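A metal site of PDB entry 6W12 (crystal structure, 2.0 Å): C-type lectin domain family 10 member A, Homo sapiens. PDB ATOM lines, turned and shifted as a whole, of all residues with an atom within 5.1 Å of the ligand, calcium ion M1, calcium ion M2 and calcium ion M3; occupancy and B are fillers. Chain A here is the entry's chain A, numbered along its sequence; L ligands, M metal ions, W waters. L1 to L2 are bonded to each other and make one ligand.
A ring nitrogen (NE2) of His 107 lies within hydrogen-bond range of an oxygen (O5) of LG2 L2.
Merely in contact with calcium ion M2: Lys 85 (3.9 Å). Along chain A the residues within 4 Å of calcium ion M2 span positions 85 to 107.
ND1 of His 107 binds calcium ion M2 (2.0 Å). Water W1 is bound to calcium ion M2. Water W2 is bound to calcium ion M2, 2.2 Å away. Water W3 is bound to calcium ion M2 (2.3 Å). Calcium ion M2 has four donor atoms within binding distance.
Water W5 bridges OD2 of Asp 115 (2.8 Å) and N1 of LG2 L2 (3.0 Å).
Calcium ion M1 is bound by the side-chain carboxylate of Asp 114, the side-chain carboxylate of Glu 101, the backbone carbonyl oxygen of Asp 114, the side-chain amide oxygen of Asn 113, the side-chain carboxylate of Asp 90, the side-chain amide oxygen of Gln 88, an oxygen (O3) of LG2 L2 and an oxygen (O2) of LG2 L2. Calcium ion M1 has eight donor atoms within binding distance.
Of the 19 residues printed, 4 come within 4 Å of calcium ion M3.
The backbone NH of Asp 91 lies within hydrogen-bond range of the side-chain carboxylate of Asp 114 (2.7 Å). The side-chain carboxylate (OE1) of Glu 101 lies close to the backbone NH (N) of Trp 92 (3.2 Å). The backbone NH of Asp 102 lies within hydrogen-bond range of the backbone carbonyl oxygen of Asp 115, at 3.2 Å. N of His 105 lies within hydrogen-bond range of O of Asn 113, 2.9 Å away. OD1 of Asp 90 sits close to N of Trp 92, at 3.4 Å. OD1 of Asp 115 is in salt-bridge range of NE of Arg 119, at 2.8 Å. The side-chain carboxylate of Asp 115 sits at hydrogen-bond distance from the side-chain hydroxyl of Tyr 121, at 2.8 Å. The side-chain amino group (NZ) of Lys 85 lies within salt-bridge range of the side-chain carboxylate (OD2) of Asp 109 (2.7 Å).
Merely in contact with the ligand: Tyr 57 (3.5 Å), Trp 92 (3.6 Å), Asp 115 (3.8 Å) and His 105 (3.9 Å). Hydrophobic or aromatic side chains within 4 Å of the ligand: Tyr 57, Trp 92, His 105 and His 107. Ten residues have an atom within 4 Å of the ligand: Tyr 57, Gln 88, Asp 90, Trp 92, Glu 101, His 105, His 107, Asn 113, Asp 114 and Asp 115.
Calcium ion M3 is bound by water W4 (2.3 Å), OD1 of Asp 91 (2.3 Å), O of Glu 101 (2.4 Å), OD1 of Asp 102 (2.4 Å), water W6 (2.5 Å), OD1 of Asp 64 (2.7 Å) and OD2 of Asp 64 (2.7 Å).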
ATOM      1  N   TYR A  57      15.275   8.281   7.273  1.00  0.00           N
ATOM      2  CA  TYR A  57      16.354   8.584   8.253  1.00  0.00           C
ATOM      3  C   TYR A  57      17.691   8.059   7.735  1.00  0.00           C
ATOM      4  O   TYR A  57      17.744   6.908   7.288  1.00  0.00           O
ATOM      5  CB  TYR A  57      16.049   7.980   9.615  1.00  0.00           C
ATOM      6  CG  TYR A  57      14.816   8.525  10.279  1.00  0.00           C
ATOM      7  CD1 TYR A  57      14.401   9.829  10.045  1.00  0.00           C
ATOM      8  CD2 TYR A  57      14.014   7.720  11.078  1.00  0.00           C
ATOM      9  CE1 TYR A  57      13.255  10.329  10.618  1.00  0.00           C
ATOM     10  CE2 TYR A  57      12.849   8.210  11.663  1.00  0.00           C
ATOM     11  CZ  TYR A  57      12.485   9.526  11.447  1.00  0.00           C
ATOM     12  OH  TYR A  57      11.359  10.045  12.008  1.00  0.00           O
ATOM     13  N   ASP A  64      28.577  10.258  19.822  1.00  0.00           N
ATOM     14  CA  ASP A  64      29.116  10.671  21.152  1.00  0.00           C
ATOM     15  C   ASP A  64      29.153   9.514  22.159  1.00  0.00           C
ATOM     16  O   ASP A  64      28.798   9.687  23.312  1.00  0.00           O
ATOM     17  CB  ASP A  64      28.316  11.834  21.721  1.00  0.00           C
ATOM     18  CG  ASP A  64      26.943  11.466  22.228  1.00  0.00           C
ATOM     19  OD1 ASP A  64      26.416  10.422  21.802  1.00  0.00           O
ATOM     20  OD2 ASP A  64      26.406  12.201  23.099  1.00  0.00           O
ATOM     21  N   TRP A  69      30.471  14.786  21.401  1.00  0.00           N
ATOM     22  CA  TRP A  69      30.147  14.618  19.948  1.00  0.00           C
ATOM     23  C   TRP A  69      31.433  14.685  19.143  1.00  0.00           C
ATOM     24  O   TRP A  69      32.204  15.605  19.329  1.00  0.00           O
ATOM     25  CB  TRP A  69      29.136  15.651  19.460  1.00  0.00           C
ATOM     26  CG  TRP A  69      27.783  15.315  19.994  1.00  0.00           C
ATOM     27  CD1 TRP A  69      27.154  15.833  21.092  1.00  0.00           C
ATOM     28  CD2 TRP A  69      26.923  14.292  19.476  1.00  0.00           C
ATOM     29  NE1 TRP A  69      25.953  15.205  21.280  1.00  0.00           N
ATOM     30  CE2 TRP A  69      25.768  14.267  20.295  1.00  0.00           C
ATOM     31  CE3 TRP A  69      27.004  13.420  18.398  1.00  0.00           C
ATOM     32  CZ2 TRP A  69      24.735  13.373  20.075  1.00  0.00           C
ATOM     33  CZ3 TRP A  69      25.972  12.537  18.187  1.00  0.00           C
ATOM     34  CH2 TRP A  69      24.857  12.512  19.015  1.00  0.00           C
ATOM     35  N   LYS A  85      17.612  19.248  14.992  1.00  0.00           N
ATOM     36  CA  LYS A  85      16.148  19.432  15.215  1.00  0.00           C
ATOM     37  C   LYS A  85      15.974  20.170  16.545  1.00  0.00           C
ATOM     38  O   LYS A  85      16.774  19.984  17.445  1.00  0.00           O
ATOM     39  CB  LYS A  85      15.398  18.100  15.315  1.00  0.00           C
ATOM     40  CG  LYS A  85      14.891  17.500  14.017  1.00  0.00           C
ATOM     41  CD  LYS A  85      13.581  18.077  13.497  1.00  0.00           C
ATOM     42  CE  LYS A  85      13.135  17.379  12.223  1.00  0.00           C
ATOM     43  NZ  LYS A  85      12.088  18.124  11.484  1.00  0.00           N
ATOM     44  N   GLN A  88      16.914  18.629  20.137  1.00  0.00           N
ATOM     45  CA  GLN A  88      17.975  17.602  19.952  1.00  0.00           C
ATOM     46  C   GLN A  88      19.315  18.312  20.065  1.00  0.00           C
ATOM     47  O   GLN A  88      19.421  19.520  19.841  1.00  0.00           O
ATOM     48  CB  GLN A  88      17.778  16.863  18.633  1.00  0.00           C
ATOM     49  CG  GLN A  88      16.344  16.368  18.438  1.00  0.00           C
ATOM     50  CD  GLN A  88      15.949  15.266  19.395  1.00  0.00           C
ATOM     51  OE1 GLN A  88      16.785  14.686  20.090  1.00  0.00           O
ATOM     52  NE2 GLN A  88      14.663  14.960  19.475  1.00  0.00           N
ATOM     53  N   ASP A  90      19.163  15.014  22.673  1.00  0.00           N
ATOM     54  CA  ASP A  90      18.535  14.856  24.006  1.00  0.00           C
ATOM     55  C   ASP A  90      19.044  13.593  24.695  1.00  0.00           C
ATOM     56  O   ASP A  90      18.669  13.404  25.832  1.00  0.00           O
ATOM     57  CB  ASP A  90      17.011  14.908  23.898  1.00  0.00           C
ATOM     58  CG  ASP A  90      16.410  13.815  23.046  1.00  0.00           C
ATOM     59  OD1 ASP A  90      17.216  13.040  22.441  1.00  0.00           O
ATOM     60  OD2 ASP A  90      15.160  13.684  23.033  1.00  0.00           O
ATOM     61  N   ASP A  91      19.829  12.723  24.037  1.00  0.00           N
ATOM     62  CA  ASP A  91      20.345  11.465  24.645  1.00  0.00           C
ATOM     63  C   ASP A  91      19.157  10.674  25.265  1.00  0.00           C
ATOM     64  O   ASP A  91      19.305  10.169  26.397  1.00  0.00           O
ATOM     65  CB  ASP A  91      21.426  11.742  25.697  1.00  0.00           C
ATOM     66  CG  ASP A  91      22.304  10.539  26.040  1.00  0.00           C
ATOM     67  OD1 ASP A  91      22.729   9.809  25.103  1.00  0.00           O
ATOM     68  OD2 ASP A  91      22.631  10.368  27.215  1.00  0.00           O
ATOM     69  N   TRP A  92      18.036  10.560  24.565  1.00  0.00           N
ATOM     70  CA  TRP A  92      16.766  10.015  25.120  1.00  0.00           C
ATOM     71  C   TRP A  92      16.968   8.563  25.571  1.00  0.00           C
ATOM     72  O   TRP A  92      17.609   7.807  24.809  1.00  0.00           O
ATOM     73  CB  TRP A  92      15.673  10.099  24.085  1.00  0.00           C
ATOM     74  CG  TRP A  92      14.298   9.767  24.530  1.00  0.00           C
ATOM     75  CD1 TRP A  92      13.607  10.273  25.591  1.00  0.00           C
ATOM     76  CD2 TRP A  92      13.380   8.932  23.821  1.00  0.00           C
ATOM     77  NE1 TRP A  92      12.329   9.783  25.602  1.00  0.00           N
ATOM     78  CE2 TRP A  92      12.171   8.949  24.529  1.00  0.00           C
ATOM     79  CE3 TRP A  92      13.488   8.164  22.645  1.00  0.00           C
ATOM     80  CZ2 TRP A  92      11.061   8.241  24.098  1.00  0.00           C
ATOM     81  CZ3 TRP A  92      12.388   7.477  22.223  1.00  0.00           C
ATOM     82  CH2 TRP A  92      11.200   7.486  22.960  1.00  0.00           C
ATOM     83  N   GLU A 101      21.209   7.876  23.472  1.00  0.00           N
ATOM     84  CA  GLU A 101      21.203   7.909  21.986  1.00  0.00           C
ATOM     85  C   GLU A 101      22.547   8.473  21.567  1.00  0.00           C
ATOM     86  O   GLU A 101      22.864   9.595  21.975  1.00  0.00           O
ATOM     87  CB  GLU A 101      20.062   8.799  21.481  1.00  0.00           C
ATOM     88  CG  GLU A 101      18.680   8.169  21.665  1.00  0.00           C
ATOM     89  CD  GLU A 101      17.541   9.052  21.200  1.00  0.00           C
ATOM     90  OE1 GLU A 101      17.640  10.270  21.417  1.00  0.00           O
ATOM     91  OE2 GLU A 101      16.583   8.521  20.552  1.00  0.00           O
ATOM     92  N   ASP A 102      23.359   7.748  20.808  1.00  0.00           N
ATOM     93  CA  ASP A 102      24.761   8.188  20.636  1.00  0.00           C
ATOM     94  C   ASP A 102      25.115   8.385  19.168  1.00  0.00           C
ATOM     95  O   ASP A 102      26.267   8.689  18.923  1.00  0.00           O
ATOM     96  CB  ASP A 102      25.718   7.217  21.302  1.00  0.00           C
ATOM     97  CG  ASP A 102      25.545   7.105  22.819  1.00  0.00           C
ATOM     98  OD1 ASP A 102      24.939   8.053  23.447  1.00  0.00           O
ATOM     99  OD2 ASP A 102      25.937   6.080  23.346  1.00  0.00           O
ATOM    100  N   HIS A 105      21.584  11.253  12.891  1.00  0.00           N
ATOM    101  CA  HIS A 105      21.044  11.030  11.538  1.00  0.00           C
ATOM    102  C   HIS A 105      20.292  12.247  11.070  1.00  0.00           C
ATOM    103  O   HIS A 105      19.843  13.070  11.912  1.00  0.00           O
ATOM    104  CB  HIS A 105      20.139   9.788  11.497  1.00  0.00           C
ATOM    105  CG  HIS A 105      18.892   9.961  12.286  1.00  0.00           C
ATOM    106  ND1 HIS A 105      17.710  10.384  11.692  1.00  0.00           N
ATOM    107  CD2 HIS A 105      18.643   9.805  13.607  1.00  0.00           C
ATOM    108  CE1 HIS A 105      16.758  10.448  12.630  1.00  0.00           C
ATOM    109  NE2 HIS A 105      17.307  10.120  13.828  1.00  0.00           N
ATOM    110  N   HIS A 107      16.876  13.735   9.562  1.00  0.00           N
ATOM    111  CA  HIS A 107      15.454  13.659   9.179  1.00  0.00           C
ATOM    112  C   HIS A 107      15.386  13.981   7.686  1.00  0.00           C
ATOM    113  O   HIS A 107      16.306  14.564   7.138  1.00  0.00           O
ATOM    114  CB  HIS A 107      14.582  14.627   9.974  1.00  0.00           C
ATOM    115  CG  HIS A 107      14.126  14.099  11.306  1.00  0.00           C
ATOM    116  ND1 HIS A 107      12.786  14.021  11.643  1.00  0.00           N
ATOM    117  CD2 HIS A 107      14.822  13.684  12.375  1.00  0.00           C
ATOM    118  CE1 HIS A 107      12.687  13.550  12.880  1.00  0.00           C
ATOM    119  NE2 HIS A 107      13.933  13.341  13.357  1.00  0.00           N
ATOM    120  N   PRO A 108      14.316  13.586   6.983  1.00  0.00           N
ATOM    121  CA  PRO A 108      14.140  13.963   5.570  1.00  0.00           C
ATOM    122  C   PRO A 108      14.251  15.456   5.237  1.00  0.00           C
ATOM    123  O   PRO A 108      14.697  15.759   4.151  1.00  0.00           O
ATOM    124  CB  PRO A 108      12.714  13.453   5.296  1.00  0.00           C
ATOM    125  CG  PRO A 108      12.638  12.218   6.171  1.00  0.00           C
ATOM    126  CD  PRO A 108      13.275  12.679   7.475  1.00  0.00           C
ATOM    127  N   ASP A 109      13.885  16.345   6.162  1.00  0.00           N
ATOM    128  CA  ASP A 109      14.002  17.830   6.021  1.00  0.00           C
ATOM    129  C   ASP A 109      15.457  18.277   6.238  1.00  0.00           C
ATOM    130  O   ASP A 109      15.727  19.463   6.111  1.00  0.00           O
ATOM    131  CB  ASP A 109      13.047  18.567   6.974  1.00  0.00           C
ATOM    132  CG  ASP A 109      13.502  18.626   8.430  1.00  0.00           C
ATOM    133  OD1 ASP A 109      14.387  17.854   8.785  1.00  0.00           O
ATOM    134  OD2 ASP A 109      12.932  19.426   9.227  1.00  0.00           O
ATOM    135  N   ASN A 113      19.071  14.479  14.379  1.00  0.00           N
ATOM    136  CA  ASN A 113      18.603  13.856  15.637  1.00  0.00           C
ATOM    137  C   ASN A 113      19.673  12.873  16.111  1.00  0.00           C
ATOM    138  O   ASN A 113      20.311  12.231  15.261  1.00  0.00           O
ATOM    139  CB  ASN A 113      17.251  13.173  15.463  1.00  0.00           C
ATOM    140  CG  ASN A 113      16.862  12.368  16.681  1.00  0.00           C
ATOM    141  OD1 ASN A 113      16.783  12.920  17.770  1.00  0.00           O
ATOM    142  ND2 ASN A 113      16.644  11.073  16.512  1.00  0.00           N
ATOM    143  N   ASP A 114      19.834  12.750  17.417  1.00  0.00           N
ATOM    144  CA  ASP A 114      20.560  11.645  18.050  1.00  0.00           C
ATOM    145  C   ASP A 114      19.623  10.449  18.267  1.00  0.00           C
ATOM    146  O   ASP A 114      18.528  10.635  18.790  1.00  0.00           O
ATOM    147  CB  ASP A 114      21.277  12.103  19.301  1.00  0.00           C
ATOM    148  CG  ASP A 114      20.418  12.651  20.424  1.00  0.00           C
ATOM    149  OD1 ASP A 114      19.256  13.084  20.130  1.00  0.00           O
ATOM    150  OD2 ASP A 114      20.905  12.592  21.596  1.00  0.00           O
ATOM    151  N   ASP A 115      20.049   9.226  17.904  1.00  0.00           N
ATOM    152  CA  ASP A 115      19.169   8.043  18.008  1.00  0.00           C
ATOM    153  C   ASP A 115      20.038   6.864  18.421  1.00  0.00           C
ATOM    154  O   ASP A 115      21.261   7.011  18.524  1.00  0.00           O
ATOM    155  CB  ASP A 115      18.469   7.770  16.674  1.00  0.00           C
ATOM    156  CG  ASP A 115      17.065   7.195  16.785  1.00  0.00           C
ATOM    157  OD1 ASP A 115      16.865   6.327  17.630  1.00  0.00           O
ATOM    158  OD2 ASP A 115      16.157   7.607  15.983  1.00  0.00           O
ATOM    159  N   ARG A 119      19.963   1.093  15.244  1.00  0.00           N
ATOM    160  CA  ARG A 119      18.832   1.131  14.273  1.00  0.00           C
ATOM    161  C   ARG A 119      19.359   1.012  12.851  1.00  0.00           C
ATOM    162  O   ARG A 119      20.365   1.647  12.488  1.00  0.00           O
ATOM    163  CB  ARG A 119      17.999   2.408  14.435  1.00  0.00           C
ATOM    164  CG  ARG A 119      17.341   2.534  15.810  1.00  0.00           C
ATOM    165  CD  ARG A 119      16.192   3.502  15.731  1.00  0.00           C
ATOM    166  NE  ARG A 119      15.670   3.854  17.037  1.00  0.00           N
ATOM    167  CZ  ARG A 119      14.805   3.152  17.732  1.00  0.00           C
ATOM    168  NH1 ARG A 119      14.347   2.004  17.250  1.00  0.00           N
ATOM    169  NH2 ARG A 119      14.450   3.589  18.937  1.00  0.00           N
ATOM    170  N   TYR A 121      19.381   2.320   9.576  1.00  0.00           N
ATOM    171  CA  TYR A 121      19.050   3.519   8.785  1.00  0.00           C
ATOM    172  C   TYR A 121      19.871   3.480   7.499  1.00  0.00           C
ATOM    173  O   TYR A 121      20.922   2.810   7.391  1.00  0.00           O
ATOM    174  CB  TYR A 121      19.318   4.768   9.617  1.00  0.00           C
ATOM    175  CG  TYR A 121      18.351   5.085  10.739  1.00  0.00           C
ATOM    176  CD1 TYR A 121      17.085   4.537  10.793  1.00  0.00           C
ATOM    177  CD2 TYR A 121      18.695   6.032  11.698  1.00  0.00           C
ATOM    178  CE1 TYR A 121      16.183   4.886  11.780  1.00  0.00           C
ATOM    179  CE2 TYR A 121      17.793   6.431  12.692  1.00  0.00           C
ATOM    180  CZ  TYR A 121      16.527   5.843  12.729  1.00  0.00           C
ATOM    181  OH  TYR A 121      15.604   6.179  13.678  1.00  0.00           O
HETATM  182  N1  LIG L   1       9.153   8.883  19.752  1.00  0.00           N
HETATM  183  C1  LIG L   1       9.686   8.362  18.467  1.00  0.00           C
HETATM  184  C2  LIG L   1      10.021   6.864  18.655  1.00  0.00           C
HETATM  185  O1  LIG L   1       9.172   5.958  18.540  1.00  0.00           O
HETATM  186  C3  LIG L   1      10.787   9.323  18.009  1.00  0.00           C
HETATM  187  O2  LIG L   1      11.196  10.188  19.082  1.00  0.00           O
HETATM  188  O3  LIG L   1      11.133   6.441  18.960  1.00  0.00           O
HETATM  189  O1  LG2 L   2      11.851  12.204  19.942  1.00  0.00           O
HETATM  190  C1  LG2 L   2      11.870  11.395  18.772  1.00  0.00           C
HETATM  191  C2  LG2 L   2      13.350  11.172  18.401  1.00  0.00           C
HETATM  192  N1  LG2 L   2      13.526  10.440  17.160  1.00  0.00           N
HETATM  193  C3  LG2 L   2      14.129  10.500  19.534  1.00  0.00           C
HETATM  194  O2  LG2 L   2      15.512  10.402  19.248  1.00  0.00           O
HETATM  195  C4  LG2 L   2      13.945  11.266  20.843  1.00  0.00           C
HETATM  196  O3  LG2 L   2      14.747  12.450  20.770  1.00  0.00           O
HETATM  197  C5  LG2 L   2      12.460  11.551  21.070  1.00  0.00           C
HETATM  198  C6  LG2 L   2      12.222  12.420  22.283  1.00  0.00           C
HETATM  199  O4  LG2 L   2      10.897  12.281  22.754  1.00  0.00           O
HETATM  200  C7  LG2 L   2      13.566  11.012  15.948  1.00  0.00           C
HETATM  201  O5  LG2 L   2      13.685  12.227  15.804  1.00  0.00           O
HETATM  202  C8  LG2 L   2      13.505  10.083  14.778  1.00  0.00           C
HETATM  203 CA    CA M   1      17.169  12.214  20.091  1.00  0.00          CA
HETATM  204 CA    CA M   2      11.149  14.508  10.548  1.00  0.00          CA
HETATM  205 CA    CA M   3      24.431  10.417  23.627  1.00  0.00          CA
HETATM  206  O   HOH W   1      11.431  15.927   8.922  1.00  0.00           O
HETATM  207  O   HOH W   2       9.884  15.397  12.182  1.00  0.00           O
HETATM  208  O   HOH W   3      10.247  12.560   9.831  1.00  0.00           O
HETATM  209  O   HOH W   4      23.282  12.313  23.036  1.00  0.00           O
HETATM  210  O   HOH W   5      13.673   7.435  17.163  1.00  0.00           O
HETATM  211  O   HOH W   6      26.196  10.130  25.317  1.00  0.00           O
